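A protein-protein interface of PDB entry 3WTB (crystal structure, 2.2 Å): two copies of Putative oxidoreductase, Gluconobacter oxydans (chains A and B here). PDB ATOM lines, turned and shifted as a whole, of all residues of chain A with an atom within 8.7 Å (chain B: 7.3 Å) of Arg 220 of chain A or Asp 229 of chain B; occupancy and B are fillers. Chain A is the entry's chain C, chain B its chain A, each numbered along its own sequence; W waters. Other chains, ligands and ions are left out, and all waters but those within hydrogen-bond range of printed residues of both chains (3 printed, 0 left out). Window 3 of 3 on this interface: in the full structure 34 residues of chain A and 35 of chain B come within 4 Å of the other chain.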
ATOM      1  N   ILE A  18      -5.101 -19.059  11.606  1.00  0.00           N
ATOM      2  CA  ILE A  18      -5.243 -17.764  10.953  1.00  0.00           C
ATOM      3  C   ILE A  18      -4.973 -16.666  11.953  1.00  0.00           C
ATOM      4  O   ILE A  18      -4.274 -15.701  11.666  1.00  0.00           O
ATOM      5  CB  ILE A  18      -6.670 -17.631  10.411  1.00  0.00           C
ATOM      6  CG1 ILE A  18      -6.940 -18.788   9.444  1.00  0.00           C
ATOM      7  CG2 ILE A  18      -6.919 -16.252   9.835  1.00  0.00           C
ATOM      8  CD1 ILE A  18      -7.839 -18.513   8.255  1.00  0.00           C
ATOM      9  N   ALA A  21      -1.285 -16.174  12.680  1.00  0.00           N
ATOM     10  CA  ALA A  21      -0.582 -15.561  11.539  1.00  0.00           C
ATOM     11  C   ALA A  21      -0.939 -14.025  11.491  1.00  0.00           C
ATOM     12  O   ALA A  21      -0.089 -13.183  11.185  1.00  0.00           O
ATOM     13  CB  ALA A  21      -1.013 -16.277  10.276  1.00  0.00           C
ATOM     14  N   ILE A  22      -2.200 -13.668  11.801  1.00  0.00           N
ATOM     15  CA  ILE A  22      -2.587 -12.263  11.824  1.00  0.00           C
ATOM     16  C   ILE A  22      -1.811 -11.543  12.894  1.00  0.00           C
ATOM     17  O   ILE A  22      -1.307 -10.433  12.698  1.00  0.00           O
ATOM     18  CB  ILE A  22      -4.104 -12.134  12.081  1.00  0.00           C
ATOM     19  CG1 ILE A  22      -4.876 -12.654  10.853  1.00  0.00           C
ATOM     20  CG2 ILE A  22      -4.508 -10.692  12.386  1.00  0.00           C
ATOM     21  CD1 ILE A  22      -6.335 -12.861  11.095  1.00  0.00           C
ATOM     22  N   LYS A  25       1.790 -10.897  11.772  1.00  0.00           N
ATOM     23  CA  LYS A  25       1.833  -9.924  10.683  1.00  0.00           C
ATOM     24  C   LYS A  25       1.571  -8.536  11.221  1.00  0.00           C
ATOM     25  O   LYS A  25       2.271  -7.601  10.878  1.00  0.00           O
ATOM     26  CB  LYS A  25       0.782 -10.269   9.616  1.00  0.00           C
ATOM     27  CG  LYS A  25       0.901  -9.407   8.367  1.00  0.00           C
ATOM     28  CD  LYS A  25       2.168  -9.759   7.571  1.00  0.00           C
ATOM     29  CE  LYS A  25       1.857 -10.759   6.425  1.00  0.00           C
ATOM     30  NZ  LYS A  25       3.059 -11.462   5.823  1.00  0.00           N
ATOM     31  N   LEU A  26       0.581  -8.383  12.118  1.00  0.00           N
ATOM     32  CA  LEU A  26       0.344  -7.029  12.680  1.00  0.00           C
ATOM     33  C   LEU A  26       1.485  -6.568  13.590  1.00  0.00           C
ATOM     34  O   LEU A  26       1.810  -5.388  13.634  1.00  0.00           O
ATOM     35  CB  LEU A  26      -0.967  -6.947  13.431  1.00  0.00           C
ATOM     36  CG  LEU A  26      -2.208  -7.159  12.605  1.00  0.00           C
ATOM     37  CD1 LEU A  26      -3.470  -7.059  13.407  1.00  0.00           C
ATOM     38  CD2 LEU A  26      -2.294  -6.232  11.454  1.00  0.00           C
ATOM     39  N   ASP A  29       3.923  -5.141  11.375  1.00  0.00           N
ATOM     40  CA  ASP A  29       3.468  -3.811  10.977  1.00  0.00           C
ATOM     41  C   ASP A  29       3.622  -2.780  12.085  1.00  0.00           C
ATOM     42  O   ASP A  29       3.436  -1.606  11.834  1.00  0.00           O
ATOM     43  CB  ASP A  29       1.990  -3.828  10.564  1.00  0.00           C
ATOM     44  CG  ASP A  29       1.717  -4.609   9.256  1.00  0.00           C
ATOM     45  OD1 ASP A  29       2.665  -4.882   8.523  1.00  0.00           O
ATOM     46  OD2 ASP A  29       0.542  -5.019   9.008  1.00  0.00           O
ATOM     47  N   VAL A 183     -13.115  -9.771   6.111  1.00  0.00           N
ATOM     48  CA  VAL A 183     -12.323 -10.630   5.281  1.00  0.00           C
ATOM     49  C   VAL A 183     -13.017 -11.976   5.208  1.00  0.00           C
ATOM     50  O   VAL A 183     -13.430 -12.498   6.238  1.00  0.00           O
ATOM     51  CB  VAL A 183     -10.931 -10.835   5.853  1.00  0.00           C
ATOM     52  CG1 VAL A 183     -10.095 -11.713   4.911  1.00  0.00           C
ATOM     53  CG2 VAL A 183     -10.261  -9.503   6.056  1.00  0.00           C
ATOM     54  N   LYS A 214      -3.547 -20.538   2.223  1.00  0.00           N
ATOM     55  CA  LYS A 214      -2.620 -20.656   3.370  1.00  0.00           C
ATOM     56  C   LYS A 214      -2.854 -19.427   4.275  1.00  0.00           C
ATOM     57  O   LYS A 214      -3.450 -18.433   3.842  1.00  0.00           O
ATOM     58  CB  LYS A 214      -1.195 -20.766   2.897  1.00  0.00           C
ATOM     59  CG  LYS A 214      -0.677 -19.552   2.108  1.00  0.00           C
ATOM     60  CD  LYS A 214       0.669 -19.851   1.426  1.00  0.00           C
ATOM     61  CE  LYS A 214       1.170 -18.600   0.675  1.00  0.00           C
ATOM     62  NZ  LYS A 214       0.308 -18.287  -0.521  1.00  0.00           N
ATOM     63  N   VAL A 215      -2.448 -19.524   5.526  1.00  0.00           N
ATOM     64  CA  VAL A 215      -2.770 -18.496   6.504  1.00  0.00           C
ATOM     65  C   VAL A 215      -2.257 -17.143   6.096  1.00  0.00           C
ATOM     66  O   VAL A 215      -2.882 -16.145   6.389  1.00  0.00           O
ATOM     67  CB  VAL A 215      -2.312 -18.868   7.946  1.00  0.00           C
ATOM     68  CG1 VAL A 215      -3.106 -20.084   8.480  1.00  0.00           C
ATOM     69  CG2 VAL A 215      -0.812 -19.168   8.038  1.00  0.00           C
ATOM     70  N   ASN A 216      -1.115 -17.088   5.432  1.00  0.00           N
ATOM     71  CA  ASN A 216      -0.560 -15.799   5.001  1.00  0.00           C
ATOM     72  C   ASN A 216      -1.492 -15.047   4.052  1.00  0.00           C
ATOM     73  O   ASN A 216      -1.483 -13.809   4.040  1.00  0.00           O
ATOM     74  CB  ASN A 216       0.798 -15.919   4.296  1.00  0.00           C
ATOM     75  CG  ASN A 216       1.522 -14.552   4.150  1.00  0.00           C
ATOM     76  OD1 ASN A 216       1.743 -13.852   5.133  1.00  0.00           O
ATOM     77  ND2 ASN A 216       1.763 -14.125   2.912  1.00  0.00           N
ATOM     78  N   ASP A 217      -2.316 -15.782   3.309  1.00  0.00           N
ATOM     79  CA  ASP A 217      -3.267 -15.130   2.388  1.00  0.00           C
ATOM     80  C   ASP A 217      -4.243 -14.230   3.187  1.00  0.00           C
ATOM     81  O   ASP A 217      -4.692 -13.190   2.685  1.00  0.00           O
ATOM     82  CB  ASP A 217      -4.060 -16.179   1.596  1.00  0.00           C
ATOM     83  CG  ASP A 217      -3.182 -17.100   0.768  1.00  0.00           C
ATOM     84  OD1 ASP A 217      -2.168 -16.623   0.190  1.00  0.00           O
ATOM     85  OD2 ASP A 217      -3.570 -18.278   0.567  1.00  0.00           O
ATOM     86  N   ILE A 218      -4.611 -14.681   4.388  1.00  0.00           N
ATOM     87  CA  ILE A 218      -5.532 -13.926   5.229  1.00  0.00           C
ATOM     88  C   ILE A 218      -4.792 -12.855   6.020  1.00  0.00           C
ATOM     89  O   ILE A 218      -5.262 -11.721   6.089  1.00  0.00           O
ATOM     90  CB  ILE A 218      -6.311 -14.834   6.193  1.00  0.00           C
ATOM     91  CG1 ILE A 218      -6.940 -15.996   5.437  1.00  0.00           C
ATOM     92  CG2 ILE A 218      -7.386 -14.052   6.930  1.00  0.00           C
ATOM     93  CD1 ILE A 218      -7.730 -15.536   4.210  1.00  0.00           C
ATOM     94  N   ALA A 219      -3.621 -13.198   6.570  1.00  0.00           N
ATOM     95  CA  ALA A 219      -2.882 -12.225   7.356  1.00  0.00           C
ATOM     96  C   ALA A 219      -2.548 -10.936   6.592  1.00  0.00           C
ATOM     97  O   ALA A 219      -2.652  -9.832   7.130  1.00  0.00           O
ATOM     98  CB  ALA A 219      -1.641 -12.834   7.909  1.00  0.00           C
ATOM     99  N   ARG A 220      -2.138 -11.114   5.344  1.00  0.00           N
ATOM    100  CA  ARG A 220      -1.751 -10.022   4.436  1.00  0.00           C
ATOM    101  C   ARG A 220      -2.956  -9.090   4.245  1.00  0.00           C
ATOM    102  O   ARG A 220      -2.799  -7.921   3.981  1.00  0.00           O
ATOM    103  CB  ARG A 220      -1.696 -10.593   3.006  1.00  0.00           C
ATOM    104  CG  ARG A 220      -0.493 -10.991   2.345  1.00  0.00           C
ATOM    105  CD  ARG A 220      -0.876 -11.386   0.928  1.00  0.00           C
ATOM    106  NE  ARG A 220      -0.567 -10.228   0.103  1.00  0.00           N
ATOM    107  CZ  ARG A 220      -1.355  -9.696  -0.796  1.00  0.00           C
ATOM    108  NH1 ARG A 220      -2.562 -10.187  -1.053  1.00  0.00           N
ATOM    109  NH2 ARG A 220      -0.910  -8.661  -1.468  1.00  0.00           N
ATOM    110  N   THR A 221      -4.134  -9.698   4.167  1.00  0.00           N
ATOM    111  CA  THR A 221      -5.333  -8.937   3.868  1.00  0.00           C
ATOM    112  C   THR A 221      -5.744  -8.102   5.082  1.00  0.00           C
ATOM    113  O   THR A 221      -6.184  -6.959   4.957  1.00  0.00           O
ATOM    114  CB  THR A 221      -6.461  -9.888   3.407  1.00  0.00           C
ATOM    115  OG1 THR A 221      -6.027 -10.701   2.290  1.00  0.00           O
ATOM    116  CG2 THR A 221      -7.703  -9.084   2.996  1.00  0.00           C
ATOM    117  N   VAL A 222      -5.626  -8.721   6.265  1.00  0.00           N
ATOM    118  CA  VAL A 222      -5.873  -8.000   7.470  1.00  0.00           C
ATOM    119  C   VAL A 222      -4.898  -6.840   7.598  1.00  0.00           C
ATOM    120  O   VAL A 222      -5.308  -5.713   7.927  1.00  0.00           O
ATOM    121  CB  VAL A 222      -5.782  -8.913   8.695  1.00  0.00           C
ATOM    122  CG1 VAL A 222      -5.962  -8.121   9.969  1.00  0.00           C
ATOM    123  CG2 VAL A 222      -6.861  -9.999   8.607  1.00  0.00           C
ATOM    124  N   SER A 223      -3.647  -7.085   7.300  1.00  0.00           N
ATOM    125  CA  SER A 223      -2.642  -6.039   7.363  1.00  0.00           C
ATOM    126  C   SER A 223      -2.992  -4.878   6.427  1.00  0.00           C
ATOM    127  O   SER A 223      -2.891  -3.679   6.791  1.00  0.00           O
ATOM    128  CB  SER A 223      -1.255  -6.654   6.973  1.00  0.00           C
ATOM    129  OG  SER A 223      -0.258  -5.664   6.849  1.00  0.00           O
ATOM    130  N   PHE A 224      -3.408  -5.209   5.202  1.00  0.00           N
ATOM    131  CA  PHE A 224      -3.809  -4.191   4.185  1.00  0.00           C
ATOM    132  C   PHE A 224      -4.971  -3.301   4.729  1.00  0.00           C
ATOM    133  O   PHE A 224      -4.970  -2.092   4.549  1.00  0.00           O
ATOM    134  CB  PHE A 224      -4.272  -4.927   2.941  1.00  0.00           C
ATOM    135  CG  PHE A 224      -4.915  -4.046   1.944  1.00  0.00           C
ATOM    136  CD1 PHE A 224      -4.149  -3.154   1.213  1.00  0.00           C
ATOM    137  CD2 PHE A 224      -6.290  -4.106   1.706  1.00  0.00           C
ATOM    138  CE1 PHE A 224      -4.745  -2.355   0.251  1.00  0.00           C
ATOM    139  CE2 PHE A 224      -6.887  -3.286   0.762  1.00  0.00           C
ATOM    140  CZ  PHE A 224      -6.121  -2.402   0.049  1.00  0.00           C
ATOM    141  N   LEU A 225      -5.949  -3.916   5.392  1.00  0.00           N
ATOM    142  CA  LEU A 225      -7.068  -3.187   5.940  1.00  0.00           C
ATOM    143  C   LEU A 225      -6.737  -2.380   7.212  1.00  0.00           C
ATOM    144  O   LEU A 225      -7.366  -1.338   7.498  1.00  0.00           O
ATOM    145  CB  LEU A 225      -8.228  -4.140   6.233  1.00  0.00           C
ATOM    146  CG  LEU A 225      -8.865  -4.802   5.029  1.00  0.00           C
ATOM    147  CD1 LEU A 225      -9.845  -5.884   5.440  1.00  0.00           C
ATOM    148  CD2 LEU A 225      -9.611  -3.765   4.214  1.00  0.00           C
ATOM    149  N   ALA A 226      -5.809  -2.879   8.004  1.00  0.00           N
ATOM    150  CA  ALA A 226      -5.506  -2.278   9.318  1.00  0.00           C
ATOM    151  C   ALA A 226      -4.593  -1.062   9.193  1.00  0.00           C
ATOM    152  O   ALA A 226      -4.473  -0.299  10.114  1.00  0.00           O
ATOM    153  CB  ALA A 226      -4.869  -3.299  10.215  1.00  0.00           C
ATOM    154  N   SER A 227      -3.983  -0.879   8.022  1.00  0.00           N
ATOM    155  CA  SER A 227      -3.118   0.235   7.775  1.00  0.00           C
ATOM    156  C   SER A 227      -3.833   1.599   7.943  1.00  0.00           C
ATOM    157  O   SER A 227      -5.013   1.712   7.646  1.00  0.00           O
ATOM    158  CB  SER A 227      -2.608   0.151   6.327  1.00  0.00           C
ATOM    159  OG  SER A 227      -1.899   1.353   5.979  1.00  0.00           O
ATOM    160  N   ILE A 238     -13.730  -8.538   1.516  1.00  0.00           N
ATOM    161  CA  ILE A 238     -12.706  -9.054   0.654  1.00  0.00           C
ATOM    162  C   ILE A 238     -12.700 -10.594   0.680  1.00  0.00           C
ATOM    163  O   ILE A 238     -12.270 -11.191   1.649  1.00  0.00           O
ATOM    164  CB  ILE A 238     -11.346  -8.499   1.029  1.00  0.00           C
ATOM    165  CG1 ILE A 238     -11.383  -6.959   0.996  1.00  0.00           C
ATOM    166  CG2 ILE A 238     -10.283  -8.978   0.046  1.00  0.00           C
ATOM    167  CD1 ILE A 238     -10.038  -6.313   1.234  1.00  0.00           C
ATOM    168  N   LEU A 239     -13.040 -11.183  -0.464  1.00  0.00           N
ATOM    169  CA  LEU A 239     -12.985 -12.627  -0.663  1.00  0.00           C
ATOM    170  C   LEU A 239     -11.553 -13.053  -0.906  1.00  0.00           C
ATOM    171  O   LEU A 239     -10.864 -12.490  -1.764  1.00  0.00           O
ATOM    172  CB  LEU A 239     -13.812 -13.004  -1.854  1.00  0.00           C
ATOM    173  CG  LEU A 239     -15.321 -12.951  -1.720  1.00  0.00           C
ATOM    174  CD1 LEU A 239     -16.005 -12.932  -3.068  1.00  0.00           C
ATOM    175  CD2 LEU A 239     -15.751 -14.151  -0.897  1.00  0.00           C
ATOM    176  N   VAL A 240     -11.082 -14.005  -0.127  1.00  0.00           N
ATOM    177  CA  VAL A 240      -9.760 -14.578  -0.296  1.00  0.00           C
ATOM    178  C   VAL A 240      -9.983 -16.065  -0.334  1.00  0.00           C
ATOM    179  O   VAL A 240      -9.803 -16.769   0.672  1.00  0.00           O
ATOM    180  CB  VAL A 240      -8.817 -14.148   0.845  1.00  0.00           C
ATOM    181  CG1 VAL A 240      -7.381 -14.629   0.585  1.00  0.00           C
ATOM    182  CG2 VAL A 240      -8.790 -12.641   0.987  1.00  0.00           C
ATOM    183  N   ARG B   7       8.667  -7.360 -14.369  1.00  0.00           N
ATOM    184  CA  ARG B   7       7.281  -7.476 -14.735  1.00  0.00           C
ATOM    185  C   ARG B   7       6.801  -6.189 -15.453  1.00  0.00           C
ATOM    186  O   ARG B   7       7.296  -5.110 -15.173  1.00  0.00           O
ATOM    187  CB  ARG B   7       6.429  -7.761 -13.507  1.00  0.00           C
ATOM    188  CG  ARG B   7       6.783  -9.074 -12.785  1.00  0.00           C
ATOM    189  CD  ARG B   7       6.104  -9.131 -11.427  1.00  0.00           C
ATOM    190  NE  ARG B   7       6.640  -8.080 -10.566  1.00  0.00           N
ATOM    191  CZ  ARG B   7       6.030  -7.586  -9.474  1.00  0.00           C
ATOM    192  NH1 ARG B   7       4.852  -8.041  -9.099  1.00  0.00           N
ATOM    193  NH2 ARG B   7       6.613  -6.616  -8.756  1.00  0.00           N
ATOM    194  N   ARG B 135      -1.927 -11.034 -13.775  1.00  0.00           N
ATOM    195  CA  ARG B 135      -2.942 -10.301 -13.022  1.00  0.00           C
ATOM    196  C   ARG B 135      -3.798  -9.490 -13.979  1.00  0.00           C
ATOM    197  O   ARG B 135      -3.279  -8.671 -14.771  1.00  0.00           O
ATOM    198  CB  ARG B 135      -2.251  -9.345 -12.059  1.00  0.00           C
ATOM    199  CG  ARG B 135      -1.351 -10.028 -11.035  1.00  0.00           C
ATOM    200  CD  ARG B 135      -2.194 -10.702 -10.005  1.00  0.00           C
ATOM    201  NE  ARG B 135      -1.465 -11.343  -8.916  1.00  0.00           N
ATOM    202  CZ  ARG B 135      -1.179 -12.647  -8.866  1.00  0.00           C
ATOM    203  NH1 ARG B 135      -1.449 -13.442  -9.883  1.00  0.00           N
ATOM    204  NH2 ARG B 135      -0.575 -13.133  -7.790  1.00  0.00           N
ATOM    205  N   SER B 223      -2.178  -2.238  -6.108  1.00  0.00           N
ATOM    206  CA  SER B 223      -0.883  -2.766  -5.770  1.00  0.00           C
ATOM    207  C   SER B 223      -1.040  -4.052  -4.934  1.00  0.00           C
ATOM    208  O   SER B 223      -0.358  -5.049  -5.149  1.00  0.00           O
ATOM    209  CB  SER B 223      -0.098  -1.687  -5.021  1.00  0.00           C
ATOM    210  OG  SER B 223       1.087  -2.201  -4.429  1.00  0.00           O
ATOM    211  N   PHE B 224      -1.979  -4.025  -3.992  1.00  0.00           N
ATOM    212  CA  PHE B 224      -2.290  -5.196  -3.145  1.00  0.00           C
ATOM    213  C   PHE B 224      -2.726  -6.428  -3.971  1.00  0.00           C
ATOM    214  O   PHE B 224      -2.285  -7.533  -3.700  1.00  0.00           O
ATOM    215  CB  PHE B 224      -3.393  -4.813  -2.167  1.00  0.00           C
ATOM    216  CG  PHE B 224      -3.930  -5.954  -1.409  1.00  0.00           C
ATOM    217  CD1 PHE B 224      -3.233  -6.456  -0.317  1.00  0.00           C
ATOM    218  CD2 PHE B 224      -5.175  -6.427  -1.649  1.00  0.00           C
ATOM    219  CE1 PHE B 224      -3.734  -7.491   0.426  1.00  0.00           C
ATOM    220  CE2 PHE B 224      -5.711  -7.452  -0.880  1.00  0.00           C
ATOM    221  CZ  PHE B 224      -4.977  -7.988   0.142  1.00  0.00           C
ATOM    222  N   LEU B 225      -3.564  -6.210  -4.981  1.00  0.00           N
ATOM    223  CA  LEU B 225      -4.012  -7.259  -5.848  1.00  0.00           C
ATOM    224  C   LEU B 225      -2.969  -7.745  -6.862  1.00  0.00           C
ATOM    225  O   LEU B 225      -2.952  -8.926  -7.242  1.00  0.00           O
ATOM    226  CB  LEU B 225      -5.247  -6.845  -6.586  1.00  0.00           C
ATOM    227  CG  LEU B 225      -6.468  -6.617  -5.735  1.00  0.00           C
ATOM    228  CD1 LEU B 225      -7.567  -5.977  -6.558  1.00  0.00           C
ATOM    229  CD2 LEU B 225      -6.977  -7.930  -5.167  1.00  0.00           C
ATOM    230  N   ALA B 226      -2.099  -6.847  -7.288  1.00  0.00           N
ATOM    231  CA  ALA B 226      -1.129  -7.170  -8.337  1.00  0.00           C
ATOM    232  C   ALA B 226       0.080  -7.942  -7.788  1.00  0.00           C
ATOM    233  O   ALA B 226       0.853  -8.507  -8.547  1.00  0.00           O
ATOM    234  CB  ALA B 226      -0.649  -5.910  -9.017  1.00  0.00           C
ATOM    235  N   SER B 227       0.263  -7.908  -6.476  1.00  0.00           N
ATOM    236  CA  SER B 227       1.331  -8.627  -5.866  1.00  0.00           C
ATOM    237  C   SER B 227       1.338 -10.110  -6.234  1.00  0.00           C
ATOM    238  O   SER B 227       0.288 -10.745  -6.303  1.00  0.00           O
ATOM    239  CB  SER B 227       1.224  -8.468  -4.326  1.00  0.00           C
ATOM    240  OG  SER B 227       2.158  -9.263  -3.665  1.00  0.00           O
ATOM    241  N   PRO B 228       2.508 -10.699  -6.403  1.00  0.00           N
ATOM    242  CA  PRO B 228       2.512 -12.174  -6.437  1.00  0.00           C
ATOM    243  C   PRO B 228       1.875 -12.862  -5.219  1.00  0.00           C
ATOM    244  O   PRO B 228       1.476 -14.016  -5.314  1.00  0.00           O
ATOM    245  CB  PRO B 228       4.032 -12.538  -6.483  1.00  0.00           C
ATOM    246  CG  PRO B 228       4.701 -11.252  -6.878  1.00  0.00           C
ATOM    247  CD  PRO B 228       3.877 -10.150  -6.308  1.00  0.00           C
ATOM    248  N   ASP B 229       1.808 -12.183  -4.074  1.00  0.00           N
ATOM    249  CA  ASP B 229       1.288 -12.824  -2.857  1.00  0.00           C
ATOM    250  C   ASP B 229      -0.199 -12.853  -2.861  1.00  0.00           C
ATOM    251  O   ASP B 229      -0.784 -13.425  -1.945  1.00  0.00           O
ATOM    252  CB  ASP B 229       1.800 -12.090  -1.599  1.00  0.00           C
ATOM    253  CG  ASP B 229       3.337 -12.190  -1.458  1.00  0.00           C
ATOM    254  OD1 ASP B 229       3.888 -13.140  -1.987  1.00  0.00           O
ATOM    255  OD2 ASP B 229       3.961 -11.361  -0.784  1.00  0.00           O
ATOM    256  N   ALA B 230      -0.814 -12.185  -3.851  1.00  0.00           N
ATOM    257  CA  ALA B 230      -2.272 -12.153  -3.973  1.00  0.00           C
ATOM    258  C   ALA B 230      -2.840 -13.302  -4.833  1.00  0.00           C
ATOM    259  O   ALA B 230      -3.908 -13.208  -5.375  1.00  0.00           O
ATOM    260  CB  ALA B 230      -2.722 -10.825  -4.545  1.00  0.00           C
ATOM    261  N   SER B 231      -2.138 -14.406  -4.876  1.00  0.00           N
ATOM    262  CA  SER B 231      -2.502 -15.537  -5.735  1.00  0.00           C
ATOM    263  C   SER B 231      -3.781 -16.235  -5.348  1.00  0.00           C
ATOM    264  O   SER B 231      -4.409 -16.868  -6.200  1.00  0.00           O
ATOM    265  CB  SER B 231      -1.299 -16.529  -5.820  1.00  0.00           C
ATOM    266  OG  SER B 231      -0.981 -17.034  -4.509  1.00  0.00           O
ATOM    267  N   TYR B 232      -4.219 -16.096  -4.075  1.00  0.00           N
ATOM    268  CA  TYR B 232      -5.439 -16.734  -3.667  1.00  0.00           C
ATOM    269  C   TYR B 232      -6.622 -15.802  -3.769  1.00  0.00           C
ATOM    270  O   TYR B 232      -7.751 -16.192  -3.431  1.00  0.00           O
ATOM    271  CB  TYR B 232      -5.296 -17.370  -2.262  1.00  0.00           C
ATOM    272  CG  TYR B 232      -6.225 -18.533  -2.026  1.00  0.00           C
ATOM    273  CD1 TYR B 232      -6.174 -19.665  -2.841  1.00  0.00           C
ATOM    274  CD2 TYR B 232      -7.191 -18.496  -1.008  1.00  0.00           C
ATOM    275  CE1 TYR B 232      -7.044 -20.733  -2.657  1.00  0.00           C
ATOM    276  CE2 TYR B 232      -8.063 -19.542  -0.856  1.00  0.00           C
ATOM    277  CZ  TYR B 232      -7.962 -20.678  -1.662  1.00  0.00           C
ATOM    278  OH  TYR B 232      -8.839 -21.741  -1.482  1.00  0.00           O
ATOM    279  N   ILE B 233      -6.404 -14.599  -4.266  1.00  0.00           N
ATOM    280  CA  ILE B 233      -7.480 -13.670  -4.460  1.00  0.00           C
ATOM    281  C   ILE B 233      -7.860 -13.638  -5.905  1.00  0.00           C
ATOM    282  O   ILE B 233      -7.133 -13.118  -6.732  1.00  0.00           O
ATOM    283  CB  ILE B 233      -7.140 -12.222  -4.011  1.00  0.00           C
ATOM    284  CG1 ILE B 233      -6.677 -12.227  -2.583  1.00  0.00           C
ATOM    285  CG2 ILE B 233      -8.378 -11.302  -4.140  1.00  0.00           C
ATOM    286  CD1 ILE B 233      -6.244 -10.902  -2.016  1.00  0.00           C
HETATM  287  O   HOH W   1      -3.039 -14.777  -1.670  1.00  0.00           O
HETATM  288  O   HOH W   2     -10.652 -14.593  -3.715  1.00  0.00           O
HETATM  289  O   HOH W   3       2.104  -9.651   0.851  1.00  0.00           O
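The guanidinium group of Arg 135 of chain B is in hydrogen-bond range of the backbone carbonyl oxygen of Ser 227 of chain B. The side-chain hydroxyl of Ser 227 of chain B lies within hydrogen-bond range of the backbone NH of Asp 229 of chain B, at 3.0 Å. The side-chain amino group (NZ) of Lys 214 of chain A lies within salt-bridge range of the side-chain carboxylate (OD1) of Asp 217 of chain A, 3.1 Å away. The backbone carbonyl oxygen (O) of Asp 217 of chain A is in hydrogen-bond range of the side-chain hydroxyl (OG1) of Thr 221 of chain A, at 2.9 Å.
Water W1 lies within hydrogen-bond range of O of Asp 229 of chain B (2.6 Å), OD1 of Asp 217 of chain A (2.8 Å), N of Tyr 232 of chain B (3.0 Å) and N of Ser 231 of chain B (3.4 Å). Water W3 lies within hydrogen-bond range of NE of Arg 220 of chain A and OD2 of Asp 229 of chain B. Water W2 bridges O of Leu 239 of chain A (2.9 Å) and O of Tyr 232 of chain B (3.3 Å).
Asp 217 of chain A touches Tyr 232 of chain B. Arg 220 of chain A touches Ser 227 of chain B (NH2 to CB, 3.6 Å). Asp 229 of chain B touches Arg 220 of chain A. CA of Ala 230 of chain B touches NH1 of Arg 220 of chain A, 3.5 Å away. Arg 220 of chain A touches Ile 233 of chain B (NH1 to CD1, 3.9 Å). Thr 221 of chain A touches Phe 224 of chain B. Phe 224 of chain A touches Phe 224 of chain B. O of Leu 239 of chain A touches CG2 of Ile 233 of chain B, 3.6 Å away. Val 240 of chain A touches Tyr 232 of chain B.
Ala 21 of chain A touches none of the printed residues of chain B. Of the printed residues of chain B, Arg 220 of chain A touches Phe 224, Ser 227, Asp 229, Ala 230 and Ile 233. Leu 225 of chain A touches none of the printed residues of chain B. Of the printed residues of chain A, Asp 229 of chain B touches Arg 220 (3.5 Å). Ala 230 of chain B touches just one residue of chain A: Arg 220. Printed residues of chain A within 4 Å of Tyr 232 of chain B: Asp 217 and Val 240. Printed residues of chain A within 4 Å of Ile 233 of chain B: Arg 220 and Leu 239. The nearest residue of chain B that does not touch Arg 220 of chain A is Leu 225 of chain B (5.0 Å).
Phe 224 of chain B touches its own counterpart, Phe 224 of chain A. Positions printed for both chains: 223, 224, 225, 226 and 227. Of the 10 pairs that touch across the chains among the printed residues, 1 has its exchanged pair printed and touching as well.
Hydrophobic or aromatic side chains of chain B that line the printed part of chain A: Phe 224, Ala 230, Tyr 232 and Ile 233. Printed residues of chain A that touch a printed residue of chain B: Asp 217, Arg 220, Thr 221, Phe 224, Leu 239 and Val 240. Hydrophobic or aromatic side chains of chain A that line the printed part of chain B: Phe 224. Among the printed residues, 10 pairs touch across the chains. Among the printed residues, no Asp or Glu carboxylate lies within 4 Å of a Lys or Arg side-chain nitrogen of the other chain.
The backbone carbonyl oxygen of Phe 224 of chain B lies within hydrogen-bond range of the guanidinium group of Arg 220 of chain A (2.9 Å).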
